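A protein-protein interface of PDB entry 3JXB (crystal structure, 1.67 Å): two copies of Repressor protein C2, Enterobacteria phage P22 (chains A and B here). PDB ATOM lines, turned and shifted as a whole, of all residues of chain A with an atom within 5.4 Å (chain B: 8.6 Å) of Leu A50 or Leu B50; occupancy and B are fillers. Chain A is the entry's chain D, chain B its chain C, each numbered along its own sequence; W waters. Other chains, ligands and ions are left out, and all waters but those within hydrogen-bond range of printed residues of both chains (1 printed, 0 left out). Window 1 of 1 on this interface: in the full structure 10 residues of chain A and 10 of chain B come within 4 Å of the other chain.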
ATOM      1  N   ASN A  45     -19.799 -10.179 -11.832  1.00  0.00           N
ATOM      2  CA  ASN A  45     -20.204 -11.514 -12.290  1.00  0.00           C
ATOM      3  C   ASN A  45     -21.616 -11.443 -12.929  1.00  0.00           C
ATOM      4  O   ASN A  45     -22.179 -10.370 -13.066  1.00  0.00           O
ATOM      5  CB  ASN A  45     -20.100 -12.537 -11.149  1.00  0.00           C
ATOM      6  CG  ASN A  45     -21.112 -12.290 -10.039  1.00  0.00           C
ATOM      7  OD1 ASN A  45     -22.083 -11.590 -10.247  1.00  0.00           O
ATOM      8  ND2 ASN A  45     -20.880 -12.870  -8.857  1.00  0.00           N
ATOM      9  N   GLY A  46     -22.186 -12.580 -13.294  1.00  0.00           N
ATOM     10  CA  GLY A  46     -23.430 -12.580 -14.047  1.00  0.00           C
ATOM     11  C   GLY A  46     -24.536 -11.928 -13.259  1.00  0.00           C
ATOM     12  O   GLY A  46     -25.181 -10.971 -13.711  1.00  0.00           O
ATOM     13  N   GLU A  47     -24.752 -12.439 -12.057  1.00  0.00           N
ATOM     14  CA  GLU A  47     -25.871 -11.947 -11.261  1.00  0.00           C
ATOM     15  C   GLU A  47     -25.718 -10.450 -10.908  1.00  0.00           C
ATOM     16  O   GLU A  47     -26.700  -9.659 -10.944  1.00  0.00           O
ATOM     17  CB  GLU A  47     -26.119 -12.861 -10.053  1.00  0.00           C
ATOM     18  CG  GLU A  47     -25.165 -12.790  -8.908  1.00  0.00           C
ATOM     19  CD  GLU A  47     -25.674 -13.670  -7.742  1.00  0.00           C
ATOM     20  OE1 GLU A  47     -26.814 -14.197  -7.818  1.00  0.00           O
ATOM     21  OE2 GLU A  47     -24.931 -13.844  -6.758  1.00  0.00           O
ATOM     22  N   ASN A  48     -24.493 -10.067 -10.581  1.00  0.00           N
ATOM     23  CA  ASN A  48     -24.211  -8.662 -10.205  1.00  0.00           C
ATOM     24  C   ASN A  48     -24.293  -7.727 -11.400  1.00  0.00           C
ATOM     25  O   ASN A  48     -24.732  -6.581 -11.256  1.00  0.00           O
ATOM     26  CB  ASN A  48     -22.854  -8.537  -9.472  1.00  0.00           C
ATOM     27  CG  ASN A  48     -22.849  -9.235  -8.134  1.00  0.00           C
ATOM     28  OD1 ASN A  48     -23.899  -9.382  -7.480  1.00  0.00           O
ATOM     29  ND2 ASN A  48     -21.679  -9.702  -7.718  1.00  0.00           N
ATOM     30  N   LEU A  49     -23.876  -8.182 -12.580  1.00  0.00           N
ATOM     31  CA  LEU A  49     -24.028  -7.341 -13.774  1.00  0.00           C
ATOM     32  C   LEU A  49     -25.500  -7.044 -14.044  1.00  0.00           C
ATOM     33  O   LEU A  49     -25.868  -5.909 -14.332  1.00  0.00           O
ATOM     34  CB  LEU A  49     -23.382  -7.974 -15.028  1.00  0.00           C
ATOM     35  CG  LEU A  49     -23.609  -7.184 -16.345  1.00  0.00           C
ATOM     36  CD1 LEU A  49     -22.977  -5.765 -16.315  1.00  0.00           C
ATOM     37  CD2 LEU A  49     -23.043  -7.958 -17.494  1.00  0.00           C
ATOM     38  N   LEU A  50     -26.357  -8.054 -13.928  1.00  0.00           N
ATOM     39  CA  LEU A  50     -27.770  -7.800 -14.186  1.00  0.00           C
ATOM     40  C   LEU A  50     -28.381  -6.889 -13.129  1.00  0.00           C
ATOM     41  O   LEU A  50     -29.141  -5.996 -13.472  1.00  0.00           O
ATOM     42  CB  LEU A  50     -28.563  -9.100 -14.399  1.00  0.00           C
ATOM     43  CG  LEU A  50     -28.546  -9.655 -15.835  1.00  0.00           C
ATOM     44  CD1 LEU A  50     -29.515  -8.932 -16.715  1.00  0.00           C
ATOM     45  CD2 LEU A  50     -27.177  -9.607 -16.488  1.00  0.00           C
ATOM     46  N   ALA A  51     -28.021  -7.089 -11.862  1.00  0.00           N
ATOM     47  CA  ALA A  51     -28.492  -6.208 -10.775  1.00  0.00           C
ATOM     48  C   ALA A  51     -27.988  -4.778 -10.936  1.00  0.00           C
ATOM     49  O   ALA A  51     -28.722  -3.796 -10.707  1.00  0.00           O
ATOM     50  CB  ALA A  51     -28.043  -6.765  -9.429  1.00  0.00           C
ATOM     51  N   LEU A  52     -26.716  -4.657 -11.305  1.00  0.00           N
ATOM     52  CA  LEU A  52     -26.130  -3.350 -11.535  1.00  0.00           C
ATOM     53  C   LEU A  52     -26.819  -2.597 -12.673  1.00  0.00           C
ATOM     54  O   LEU A  52     -27.058  -1.402 -12.553  1.00  0.00           O
ATOM     55  CB  LEU A  52     -24.632  -3.500 -11.794  1.00  0.00           C
ATOM     56  CG  LEU A  52     -23.797  -2.260 -12.139  1.00  0.00           C
ATOM     57  CD1 LEU A  52     -23.708  -1.327 -10.939  1.00  0.00           C
ATOM     58  CD2 LEU A  52     -22.402  -2.713 -12.622  1.00  0.00           C
ATOM     59  N   SER A  53     -27.105  -3.294 -13.776  1.00  0.00           N
ATOM     60  CA  SER A  53     -27.789  -2.669 -14.910  1.00  0.00           C
ATOM     61  C   SER A  53     -29.165  -2.130 -14.522  1.00  0.00           C
ATOM     62  O   SER A  53     -29.561  -1.062 -14.991  1.00  0.00           O
ATOM     63  CB  SER A  53     -27.899  -3.626 -16.103  1.00  0.00           C
ATOM     64  OG  SER A  53     -28.730  -4.731 -15.812  1.00  0.00           O
ATOM     65  N   LYS A  54     -29.898  -2.875 -13.684  1.00  0.00           N
ATOM     66  CA  LYS A  54     -31.200  -2.433 -13.202  1.00  0.00           C
ATOM     67  C   LYS A  54     -31.078  -1.196 -12.310  1.00  0.00           C
ATOM     68  O   LYS A  54     -31.867  -0.260 -12.454  1.00  0.00           O
ATOM     69  CB  LYS A  54     -31.958  -3.572 -12.495  1.00  0.00           C
ATOM     70  CG  LYS A  54     -32.401  -4.686 -13.463  1.00  0.00           C
ATOM     71  CD  LYS A  54     -33.189  -5.805 -12.787  1.00  0.00           C
ATOM     72  CE  LYS A  54     -33.451  -6.954 -13.780  1.00  0.00           C
ATOM     73  NZ  LYS A  54     -32.171  -7.561 -14.246  1.00  0.00           N
ATOM     74  N   ALA A  55     -30.093  -1.197 -11.404  1.00  0.00           N
ATOM     75  CA  ALA A  55     -29.850  -0.052 -10.503  1.00  0.00           C
ATOM     76  C   ALA A  55     -29.464   1.203 -11.287  1.00  0.00           C
ATOM     77  O   ALA A  55     -29.822   2.319 -10.903  1.00  0.00           O
ATOM     78  CB  ALA A  55     -28.769  -0.384  -9.467  1.00  0.00           C
ATOM     79  N   PRO A  60     -27.482  -4.370 -19.667  1.00  0.00           N
ATOM     80  CA  PRO A  60     -26.155  -4.937 -19.422  1.00  0.00           C
ATOM     81  C   PRO A  60     -25.232  -4.751 -20.626  1.00  0.00           C
ATOM     82  O   PRO A  60     -24.032  -4.505 -20.441  1.00  0.00           O
ATOM     83  CB  PRO A  60     -26.425  -6.419 -19.152  1.00  0.00           C
ATOM     84  CG  PRO A  60     -27.876  -6.542 -18.921  1.00  0.00           C
ATOM     85  CD  PRO A  60     -28.564  -5.351 -19.518  1.00  0.00           C
ATOM     86  N   ASP A  61     -25.776  -4.809 -21.845  1.00  0.00           N
ATOM     87  CA  ASP A  61     -24.930  -4.599 -23.022  1.00  0.00           C
ATOM     88  C   ASP A  61     -24.338  -3.194 -23.068  1.00  0.00           C
ATOM     89  O   ASP A  61     -23.175  -3.020 -23.437  1.00  0.00           O
ATOM     90  CB  ASP A  61     -25.650  -4.941 -24.328  1.00  0.00           C
ATOM     91  CG  ASP A  61     -25.764  -6.450 -24.557  1.00  0.00           C
ATOM     92  OD1 ASP A  61     -24.865  -7.225 -24.155  1.00  0.00           O
ATOM     93  OD2 ASP A  61     -26.761  -6.867 -25.145  1.00  0.00           O
ATOM     94  N   LEU A  64     -21.377  -3.334 -20.596  1.00  0.00           N
ATOM     95  CA  LEU A  64     -20.291  -4.162 -21.106  1.00  0.00           C
ATOM     96  C   LEU A  64     -19.586  -3.560 -22.308  1.00  0.00           C
ATOM     97  O   LEU A  64     -18.358  -3.580 -22.361  1.00  0.00           O
ATOM     98  CB  LEU A  64     -20.788  -5.547 -21.493  1.00  0.00           C
ATOM     99  CG  LEU A  64     -20.917  -6.584 -20.410  1.00  0.00           C
ATOM    100  CD1 LEU A  64     -21.625  -7.751 -21.060  1.00  0.00           C
ATOM    101  CD2 LEU A  64     -19.553  -7.030 -19.847  1.00  0.00           C
ATOM    102  N   MET B  26     -19.750 -20.642 -29.587  1.00  0.00           N
ATOM    103  CA  MET B  26     -20.667 -19.526 -29.828  1.00  0.00           C
ATOM    104  C   MET B  26     -20.524 -18.455 -28.758  1.00  0.00           C
ATOM    105  O   MET B  26     -20.679 -17.278 -29.031  1.00  0.00           O
ATOM    106  CB  MET B  26     -22.117 -20.015 -29.831  1.00  0.00           C
ATOM    107  CG  MET B  26     -22.539 -20.967 -30.943  1.00  0.00           C
ATOM    108  SD  MET B  26     -24.188 -21.653 -30.599  1.00  0.00           S
ATOM    109  CE  MET B  26     -25.250 -20.298 -31.081  1.00  0.00           C
ATOM    110  N   VAL B  27     -20.206 -18.887 -27.540  1.00  0.00           N
ATOM    111  CA  VAL B  27     -20.194 -18.022 -26.366  1.00  0.00           C
ATOM    112  C   VAL B  27     -18.801 -17.437 -26.151  1.00  0.00           C
ATOM    113  O   VAL B  27     -18.664 -16.327 -25.629  1.00  0.00           O
ATOM    114  CB  VAL B  27     -20.646 -18.822 -25.137  1.00  0.00           C
ATOM    115  CG1 VAL B  27     -20.326 -18.102 -23.796  1.00  0.00           C
ATOM    116  CG2 VAL B  27     -22.151 -19.121 -25.258  1.00  0.00           C
ATOM    117  N   TRP B  37     -21.335 -24.819 -15.927  1.00  0.00           N
ATOM    118  CA  TRP B  37     -22.566 -24.032 -15.770  1.00  0.00           C
ATOM    119  C   TRP B  37     -23.793 -24.953 -15.636  1.00  0.00           C
ATOM    120  O   TRP B  37     -24.646 -24.735 -14.780  1.00  0.00           O
ATOM    121  CB  TRP B  37     -22.789 -23.064 -16.925  1.00  0.00           C
ATOM    122  CG  TRP B  37     -21.688 -22.064 -17.080  1.00  0.00           C
ATOM    123  CD1 TRP B  37     -20.732 -21.713 -16.159  1.00  0.00           C
ATOM    124  CD2 TRP B  37     -21.434 -21.282 -18.250  1.00  0.00           C
ATOM    125  NE1 TRP B  37     -19.888 -20.750 -16.699  1.00  0.00           N
ATOM    126  CE2 TRP B  37     -20.295 -20.478 -17.984  1.00  0.00           C
ATOM    127  CE3 TRP B  37     -22.056 -21.189 -19.499  1.00  0.00           C
ATOM    128  CZ2 TRP B  37     -19.768 -19.584 -18.934  1.00  0.00           C
ATOM    129  CZ3 TRP B  37     -21.533 -20.289 -20.457  1.00  0.00           C
ATOM    130  CH2 TRP B  37     -20.388 -19.521 -20.167  1.00  0.00           C
ATOM    131  N   PRO B  44     -21.870 -18.361 -15.069  1.00  0.00           N
ATOM    132  CA  PRO B  44     -21.130 -17.486 -15.984  1.00  0.00           C
ATOM    133  C   PRO B  44     -20.894 -16.084 -15.444  1.00  0.00           C
ATOM    134  O   PRO B  44     -21.755 -15.534 -14.747  1.00  0.00           O
ATOM    135  CB  PRO B  44     -22.020 -17.429 -17.224  1.00  0.00           C
ATOM    136  CG  PRO B  44     -23.379 -17.845 -16.783  1.00  0.00           C
ATOM    137  CD  PRO B  44     -23.136 -18.834 -15.660  1.00  0.00           C
ATOM    138  N   ASN B  45     -19.728 -15.525 -15.768  1.00  0.00           N
ATOM    139  CA  ASN B  45     -19.449 -14.154 -15.390  1.00  0.00           C
ATOM    140  C   ASN B  45     -20.327 -13.179 -16.222  1.00  0.00           C
ATOM    141  O   ASN B  45     -21.170 -13.617 -17.012  1.00  0.00           O
ATOM    142  CB  ASN B  45     -17.940 -13.888 -15.482  1.00  0.00           C
ATOM    143  CG  ASN B  45     -17.427 -13.810 -16.928  1.00  0.00           C
ATOM    144  OD1 ASN B  45     -18.192 -13.653 -17.872  1.00  0.00           O
ATOM    145  ND2 ASN B  45     -16.120 -13.883 -17.090  1.00  0.00           N
ATOM    146  N   GLY B  46     -20.147 -11.875 -16.044  1.00  0.00           N
ATOM    147  CA  GLY B  46     -21.017 -10.906 -16.740  1.00  0.00           C
ATOM    148  C   GLY B  46     -21.008 -11.029 -18.252  1.00  0.00           C
ATOM    149  O   GLY B  46     -22.081 -11.195 -18.876  1.00  0.00           O
ATOM    150  N   GLU B  47     -19.799 -10.941 -18.831  1.00  0.00           N
ATOM    151  CA  GLU B  47     -19.634 -11.026 -20.284  1.00  0.00           C
ATOM    152  C   GLU B  47     -20.203 -12.349 -20.787  1.00  0.00           C
ATOM    153  O   GLU B  47     -20.905 -12.390 -21.809  1.00  0.00           O
ATOM    154  CB  GLU B  47     -18.156 -10.879 -20.699  1.00  0.00           C
ATOM    155  CG  GLU B  47     -17.933 -10.908 -22.215  1.00  0.00           C
ATOM    156  CD  GLU B  47     -16.459 -10.832 -22.627  1.00  0.00           C
ATOM    157  OE1 GLU B  47     -15.579 -11.143 -21.801  1.00  0.00           O
ATOM    158  OE2 GLU B  47     -16.193 -10.502 -23.793  1.00  0.00           O
ATOM    159  N   ASN B  48     -19.883 -13.438 -20.087  1.00  0.00           N
ATOM    160  CA  ASN B  48     -20.311 -14.742 -20.586  1.00  0.00           C
ATOM    161  C   ASN B  48     -21.800 -15.001 -20.452  1.00  0.00           C
ATOM    162  O   ASN B  48     -22.386 -15.685 -21.302  1.00  0.00           O
ATOM    163  CB  ASN B  48     -19.509 -15.853 -19.919  1.00  0.00           C
ATOM    164  CG  ASN B  48     -18.038 -15.789 -20.268  1.00  0.00           C
ATOM    165  OD1 ASN B  48     -17.644 -15.235 -21.316  1.00  0.00           O
ATOM    166  ND2 ASN B  48     -17.207 -16.357 -19.399  1.00  0.00           N
ATOM    167  N   LEU B  49     -22.412 -14.454 -19.406  1.00  0.00           N
ATOM    168  CA  LEU B  49     -23.834 -14.621 -19.225  1.00  0.00           C
ATOM    169  C   LEU B  49     -24.559 -13.949 -20.418  1.00  0.00           C
ATOM    170  O   LEU B  49     -25.539 -14.489 -20.968  1.00  0.00           O
ATOM    171  CB  LEU B  49     -24.299 -14.020 -17.894  1.00  0.00           C
ATOM    172  CG  LEU B  49     -25.821 -14.008 -17.703  1.00  0.00           C
ATOM    173  CD1 LEU B  49     -26.500 -15.395 -17.858  1.00  0.00           C
ATOM    174  CD2 LEU B  49     -26.139 -13.386 -16.343  1.00  0.00           C
ATOM    175  N   LEU B  50     -24.113 -12.759 -20.799  1.00  0.00           N
ATOM    176  CA  LEU B  50     -24.787 -12.072 -21.888  1.00  0.00           C
ATOM    177  C   LEU B  50     -24.554 -12.802 -23.215  1.00  0.00           C
ATOM    178  O   LEU B  50     -25.479 -12.916 -24.050  1.00  0.00           O
ATOM    179  CB  LEU B  50     -24.398 -10.592 -21.940  1.00  0.00           C
ATOM    180  CG  LEU B  50     -25.293  -9.629 -21.133  1.00  0.00           C
ATOM    181  CD1 LEU B  50     -26.662  -9.505 -21.784  1.00  0.00           C
ATOM    182  CD2 LEU B  50     -25.445 -10.018 -19.646  1.00  0.00           C
ATOM    183  N   ALA B  51     -23.343 -13.319 -23.403  1.00  0.00           N
ATOM    184  CA  ALA B  51     -23.036 -14.060 -24.626  1.00  0.00           C
ATOM    185  C   ALA B  51     -23.869 -15.341 -24.665  1.00  0.00           C
ATOM    186  O   ALA B  51     -24.391 -15.726 -25.725  1.00  0.00           O
ATOM    187  CB  ALA B  51     -21.532 -14.379 -24.709  1.00  0.00           C
ATOM    188  N   LEU B  52     -23.958 -16.015 -23.517  1.00  0.00           N
ATOM    189  CA  LEU B  52     -24.771 -17.234 -23.417  1.00  0.00           C
ATOM    190  C   LEU B  52     -26.235 -16.971 -23.721  1.00  0.00           C
ATOM    191  O   LEU B  52     -26.870 -17.728 -24.454  1.00  0.00           O
ATOM    192  CB  LEU B  52     -24.613 -17.860 -22.037  1.00  0.00           C
ATOM    193  CG  LEU B  52     -25.509 -19.060 -21.719  1.00  0.00           C
ATOM    194  CD1 LEU B  52     -24.982 -20.243 -22.520  1.00  0.00           C
ATOM    195  CD2 LEU B  52     -25.367 -19.322 -20.250  1.00  0.00           C
ATOM    196  N   SER B  53     -26.754 -15.876 -23.185  1.00  0.00           N
ATOM    197  CA  SER B  53     -28.155 -15.525 -23.387  1.00  0.00           C
ATOM    198  C   SER B  53     -28.464 -15.278 -24.861  1.00  0.00           C
ATOM    199  O   SER B  53     -29.509 -15.671 -25.350  1.00  0.00           O
ATOM    200  CB  SER B  53     -28.546 -14.312 -22.541  1.00  0.00           C
ATOM    201  OG  SER B  53     -27.873 -13.140 -22.959  1.00  0.00           O
ATOM    202  N   LYS B  54     -27.538 -14.644 -25.565  1.00  0.00           N
ATOM    203  CA  LYS B  54     -27.725 -14.401 -26.996  1.00  0.00           C
ATOM    204  C   LYS B  54     -27.654 -15.691 -27.796  1.00  0.00           C
ATOM    205  O   LYS B  54     -28.438 -15.898 -28.728  1.00  0.00           O
ATOM    206  CB  LYS B  54     -26.686 -13.410 -27.489  1.00  0.00           C
ATOM    207  CG  LYS B  54     -26.949 -12.029 -26.911  1.00  0.00           C
ATOM    208  CD  LYS B  54     -25.920 -11.025 -27.330  1.00  0.00           C
ATOM    209  CE  LYS B  54     -26.349  -9.639 -26.879  1.00  0.00           C
ATOM    210  NZ  LYS B  54     -26.303  -9.516 -25.393  1.00  0.00           N
ATOM    211  N   ALA B  55     -26.732 -16.569 -27.411  1.00  0.00           N
ATOM    212  CA  ALA B  55     -26.579 -17.849 -28.109  1.00  0.00           C
ATOM    213  C   ALA B  55     -27.812 -18.718 -27.948  1.00  0.00           C
ATOM    214  O   ALA B  55     -28.176 -19.464 -28.866  1.00  0.00           O
ATOM    215  CB  ALA B  55     -25.335 -18.591 -27.617  1.00  0.00           C
ATOM    216  N   LEU B  56     -28.451 -18.629 -26.782  1.00  0.00           N
ATOM    217  CA  LEU B  56     -29.657 -19.419 -26.492  1.00  0.00           C
ATOM    218  C   LEU B  56     -30.981 -18.689 -26.793  1.00  0.00           C
ATOM    219  O   LEU B  56     -32.064 -19.256 -26.612  1.00  0.00           O
ATOM    220  CB  LEU B  56     -29.624 -19.917 -25.044  1.00  0.00           C
ATOM    221  CG  LEU B  56     -28.476 -20.850 -24.652  1.00  0.00           C
ATOM    222  CD1 LEU B  56     -28.588 -21.211 -23.172  1.00  0.00           C
ATOM    223  CD2 LEU B  56     -28.488 -22.106 -25.494  1.00  0.00           C
ATOM    224  N   GLN B  57     -30.886 -17.443 -27.258  1.00  0.00           N
ATOM    225  CA  GLN B  57     -32.056 -16.590 -27.482  1.00  0.00           C
ATOM    226  C   GLN B  57     -33.038 -16.546 -26.316  1.00  0.00           C
ATOM    227  O   GLN B  57     -34.257 -16.742 -26.498  1.00  0.00           O
ATOM    228  CB  GLN B  57     -32.771 -16.968 -28.782  1.00  0.00           C
ATOM    229  CG  GLN B  57     -32.154 -16.299 -29.963  1.00  0.00           C
ATOM    230  CD  GLN B  57     -32.972 -16.422 -31.200  1.00  0.00           C
ATOM    231  OE1 GLN B  57     -32.433 -16.429 -32.302  1.00  0.00           O
ATOM    232  NE2 GLN B  57     -34.289 -16.507 -31.042  1.00  0.00           N
ATOM    233  N   CYS B  58     -32.488 -16.305 -25.126  1.00  0.00           N
ATOM    234  CA  CYS B  58     -33.350 -16.008 -23.999  1.00  0.00           C
ATOM    235  C   CYS B  58     -32.778 -14.832 -23.231  1.00  0.00           C
ATOM    236  O   CYS B  58     -31.656 -14.361 -23.508  1.00  0.00           O
ATOM    237  CB  CYS B  58     -33.523 -17.229 -23.113  1.00  0.00           C
ATOM    238  SG  CYS B  58     -31.955 -17.855 -22.577  1.00  0.00           S
ATOM    239  N   SER B  59     -33.589 -14.286 -22.330  1.00  0.00           N
ATOM    240  CA  SER B  59     -33.086 -13.167 -21.561  1.00  0.00           C
ATOM    241  C   SER B  59     -32.114 -13.699 -20.523  1.00  0.00           C
ATOM    242  O   SER B  59     -32.260 -14.824 -20.033  1.00  0.00           O
ATOM    243  CB  SER B  59     -34.202 -12.368 -20.899  1.00  0.00           C
ATOM    244  OG  SER B  59     -34.671 -13.013 -19.739  1.00  0.00           O
ATOM    245  N   PRO B  60     -31.117 -12.883 -20.183  1.00  0.00           N
ATOM    246  CA  PRO B  60     -30.247 -13.254 -19.062  1.00  0.00           C
ATOM    247  C   PRO B  60     -31.043 -13.461 -17.778  1.00  0.00           C
ATOM    248  O   PRO B  60     -30.679 -14.327 -16.987  1.00  0.00           O
ATOM    249  CB  PRO B  60     -29.282 -12.069 -18.916  1.00  0.00           C
ATOM    250  CG  PRO B  60     -29.513 -11.188 -20.064  1.00  0.00           C
ATOM    251  CD  PRO B  60     -30.751 -11.603 -20.813  1.00  0.00           C
ATOM    252  N   ASP B  61     -32.131 -12.706 -17.581  1.00  0.00           N
ATOM    253  CA  ASP B  61     -32.906 -12.857 -16.344  1.00  0.00           C
ATOM    254  C   ASP B  61     -33.615 -14.214 -16.309  1.00  0.00           C
ATOM    255  O   ASP B  61     -33.713 -14.818 -15.252  1.00  0.00           O
ATOM    256  CB  ASP B  61     -33.930 -11.729 -16.136  1.00  0.00           C
ATOM    257  CG  ASP B  61     -33.275 -10.383 -15.875  1.00  0.00           C
ATOM    258  OD1 ASP B  61     -32.599 -10.205 -14.837  1.00  0.00           O
ATOM    259  OD2 ASP B  61     -33.447  -9.496 -16.722  1.00  0.00           O
ATOM    260  N   TYR B  62     -34.084 -14.698 -17.458  1.00  0.00           N
ATOM    261  CA  TYR B  62     -34.638 -16.045 -17.500  1.00  0.00           C
ATOM    262  C   TYR B  62     -33.620 -17.102 -17.063  1.00  0.00           C
ATOM    263  O   TYR B  62     -33.921 -17.954 -16.225  1.00  0.00           O
ATOM    264  CB  TYR B  62     -35.226 -16.403 -18.870  1.00  0.00           C
ATOM    265  CG  TYR B  62     -35.649 -17.864 -18.905  1.00  0.00           C
ATOM    266  CD1 TYR B  62     -36.785 -18.294 -18.212  1.00  0.00           C
ATOM    267  CD2 TYR B  62     -34.865 -18.820 -19.554  1.00  0.00           C
ATOM    268  CE1 TYR B  62     -37.155 -19.634 -18.208  1.00  0.00           C
ATOM    269  CE2 TYR B  62     -35.230 -20.170 -19.551  1.00  0.00           C
ATOM    270  CZ  TYR B  62     -36.363 -20.561 -18.881  1.00  0.00           C
ATOM    271  OH  TYR B  62     -36.731 -21.890 -18.878  1.00  0.00           O
ATOM    272  N   LEU B  63     -32.425 -17.069 -17.645  1.00  0.00           N
ATOM    273  CA  LEU B  63     -31.409 -18.026 -17.253  1.00  0.00           C
ATOM    274  C   LEU B  63     -31.058 -17.907 -15.788  1.00  0.00           C
ATOM    275  O   LEU B  63     -31.036 -18.903 -15.095  1.00  0.00           O
ATOM    276  CB  LEU B  63     -30.166 -17.893 -18.120  1.00  0.00           C
ATOM    277  CG  LEU B  63     -30.327 -18.213 -19.596  1.00  0.00           C
ATOM    278  CD1 LEU B  63     -28.976 -17.854 -20.257  1.00  0.00           C
ATOM    279  CD2 LEU B  63     -30.749 -19.688 -19.827  1.00  0.00           C
ATOM    280  N   LEU B  64     -30.763 -16.691 -15.330  1.00  0.00           N
ATOM    281  CA  LEU B  64     -30.324 -16.509 -13.951  1.00  0.00           C
ATOM    282  C   LEU B  64     -31.379 -16.919 -12.903  1.00  0.00           C
ATOM    283  O   LEU B  64     -31.068 -17.626 -11.923  1.00  0.00           O
ATOM    284  CB  LEU B  64     -29.950 -15.049 -13.726  1.00  0.00           C
ATOM    285  CG  LEU B  64     -29.159 -14.805 -12.440  1.00  0.00           C
ATOM    286  CD1 LEU B  64     -27.724 -15.320 -12.584  1.00  0.00           C
ATOM    287  CD2 LEU B  64     -29.134 -13.315 -12.076  1.00  0.00           C
ATOM    288  N   LYS B  65     -32.613 -16.449 -13.092  1.00  0.00           N
ATOM    289  CA  LYS B  65     -33.615 -16.534 -12.032  1.00  0.00           C
ATOM    290  C   LYS B  65     -34.887 -17.287 -12.405  1.00  0.00           C
ATOM    291  O   LYS B  65     -35.727 -17.557 -11.545  1.00  0.00           O
ATOM    292  CB  LYS B  65     -34.009 -15.132 -11.566  1.00  0.00           C
ATOM    293  CG  LYS B  65     -32.896 -14.328 -10.888  1.00  0.00           C
ATOM    294  CD  LYS B  65     -33.490 -13.028 -10.397  1.00  0.00           C
ATOM    295  CE  LYS B  65     -34.390 -13.203  -9.133  1.00  0.00           C
ATOM    296  NZ  LYS B  65     -35.843 -13.546  -9.339  1.00  0.00           N
HETATM  297  O   HOH W   1     -21.117 -15.557 -11.961  1.00  0.00           O
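O of Pro B44 lies within hydrogen-bond range of N of Gly A46, 3.3 Å away. NZ of Lys B54 is in salt-bridge range of OD2 of Asp A61 (2.7 Å). The side-chain carboxylate of Asp B61 lies within salt-bridge range of the side-chain amino group of Lys A54 (2.7 Å). N of Gly B46 sits close to N of Gly A46 (3.5 Å).
The side-chain amide oxygen (OD1) of Asn B45 sits at hydrogen-bond distance from the backbone NH (N) of Glu B47 (3.3 Å). N of Asp B61 lies close to OG of Ser B59 (3.3 Å). N of Asn A48 sits at hydrogen-bond distance from OD1 of Asn A45 (2.9 Å). O of Leu A49 sits at hydrogen-bond distance from OG of Ser A53 (3.4 Å). O of Leu A50 sits at hydrogen-bond distance from OG of Ser A53, 2.7 Å away. O of Leu A50 sits at hydrogen-bond distance from NZ of Lys A54 (3.5 Å).
Asn A45 touches Asn B45 (C to C, 3.9 Å). Asn A45 touches Gly B46 (C to N, 3.5 Å). Gly A46 touches Asn B45. Leu B64 touches Glu A47 (CD2 to CA, 3.6 Å). CD2 of Leu B50 touches CD2 of Leu A49, at 3.8 Å. Leu A50 touches Leu B49 (CD2 to CD2, 3.9 Å). Leu B50 touches Leu A50 (CD2 to CD2, 3.6 Å). CB of Pro B60 touches CD1 of Leu A50, at 3.8 Å. OD1 of Asp B61 touches CD1 of Leu A50 (3.8 Å). Asp A61 touches Leu B50.
Of the printed residues of chain B, Leu A50 touches Leu B49 (3.9 Å), Leu B50 (3.6 Å), Pro B60 (3.8 Å) and Asp B61 (3.8 Å). Printed residues of chain A within 4 Å of Leu B50: Leu A49, Leu A50, Pro A60 and Asp A61. No residue of chain B comes within 4 Å of Ala A51. Of the printed residues of chain B, Glu A47 touches Leu B64. Of the printed residues of chain A, Lys B54 touches Asp A61. Leu B52 touches none of the printed residues of chain A. The nearest printed residue of chain A that does not touch Leu B50 is Leu A64 (4.1 Å). The nearest printed residue of chain A that does not touch Pro B60 is Pro A60 (5.1 Å).
Of the 14 printed residues of chain A, 9 touch a printed residue of chain B. Hydrophobic or aromatic side chains of chain A that line the printed part of chain B: Leu A49, Leu A50, Pro A60 and Leu A64. Of the 25 printed residues of chain B, 10 touch a printed residue of chain A. Printed residues of chain B that touch a printed residue of chain A: Pro B44, Asn B45, Gly B46, Glu B47, Leu B49, Leu B50, Lys B54, Pro B60, Asp B61 and Leu B64. Among the printed residues, 18 pairs touch across the chains. Among the printed residues, Asp or Glu carboxylates within 4 Å of a Lys or Arg side-chain nitrogen of the other chain: Lys A54 with Asp B61 and Asp A61 with Lys B54.
Asn A45 touches Gly B46, and with the chains exchanged Gly A46 touches Asn B45. Gly A46 touches Leu B49, and with the chains exchanged Leu A49 touches Gly B46. Leu B50 touches its own counterpart, Leu A50. Leu A50 touches Pro B60, and with the chains exchanged Pro A60 touches Leu B50. Of the 18 pairs that touch across the chains among the printed residues, 17 have their exchanged pair printed and touching as well.
Water W1 lies within hydrogen-bond range of O of Pro B44 and N of Gly A46.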
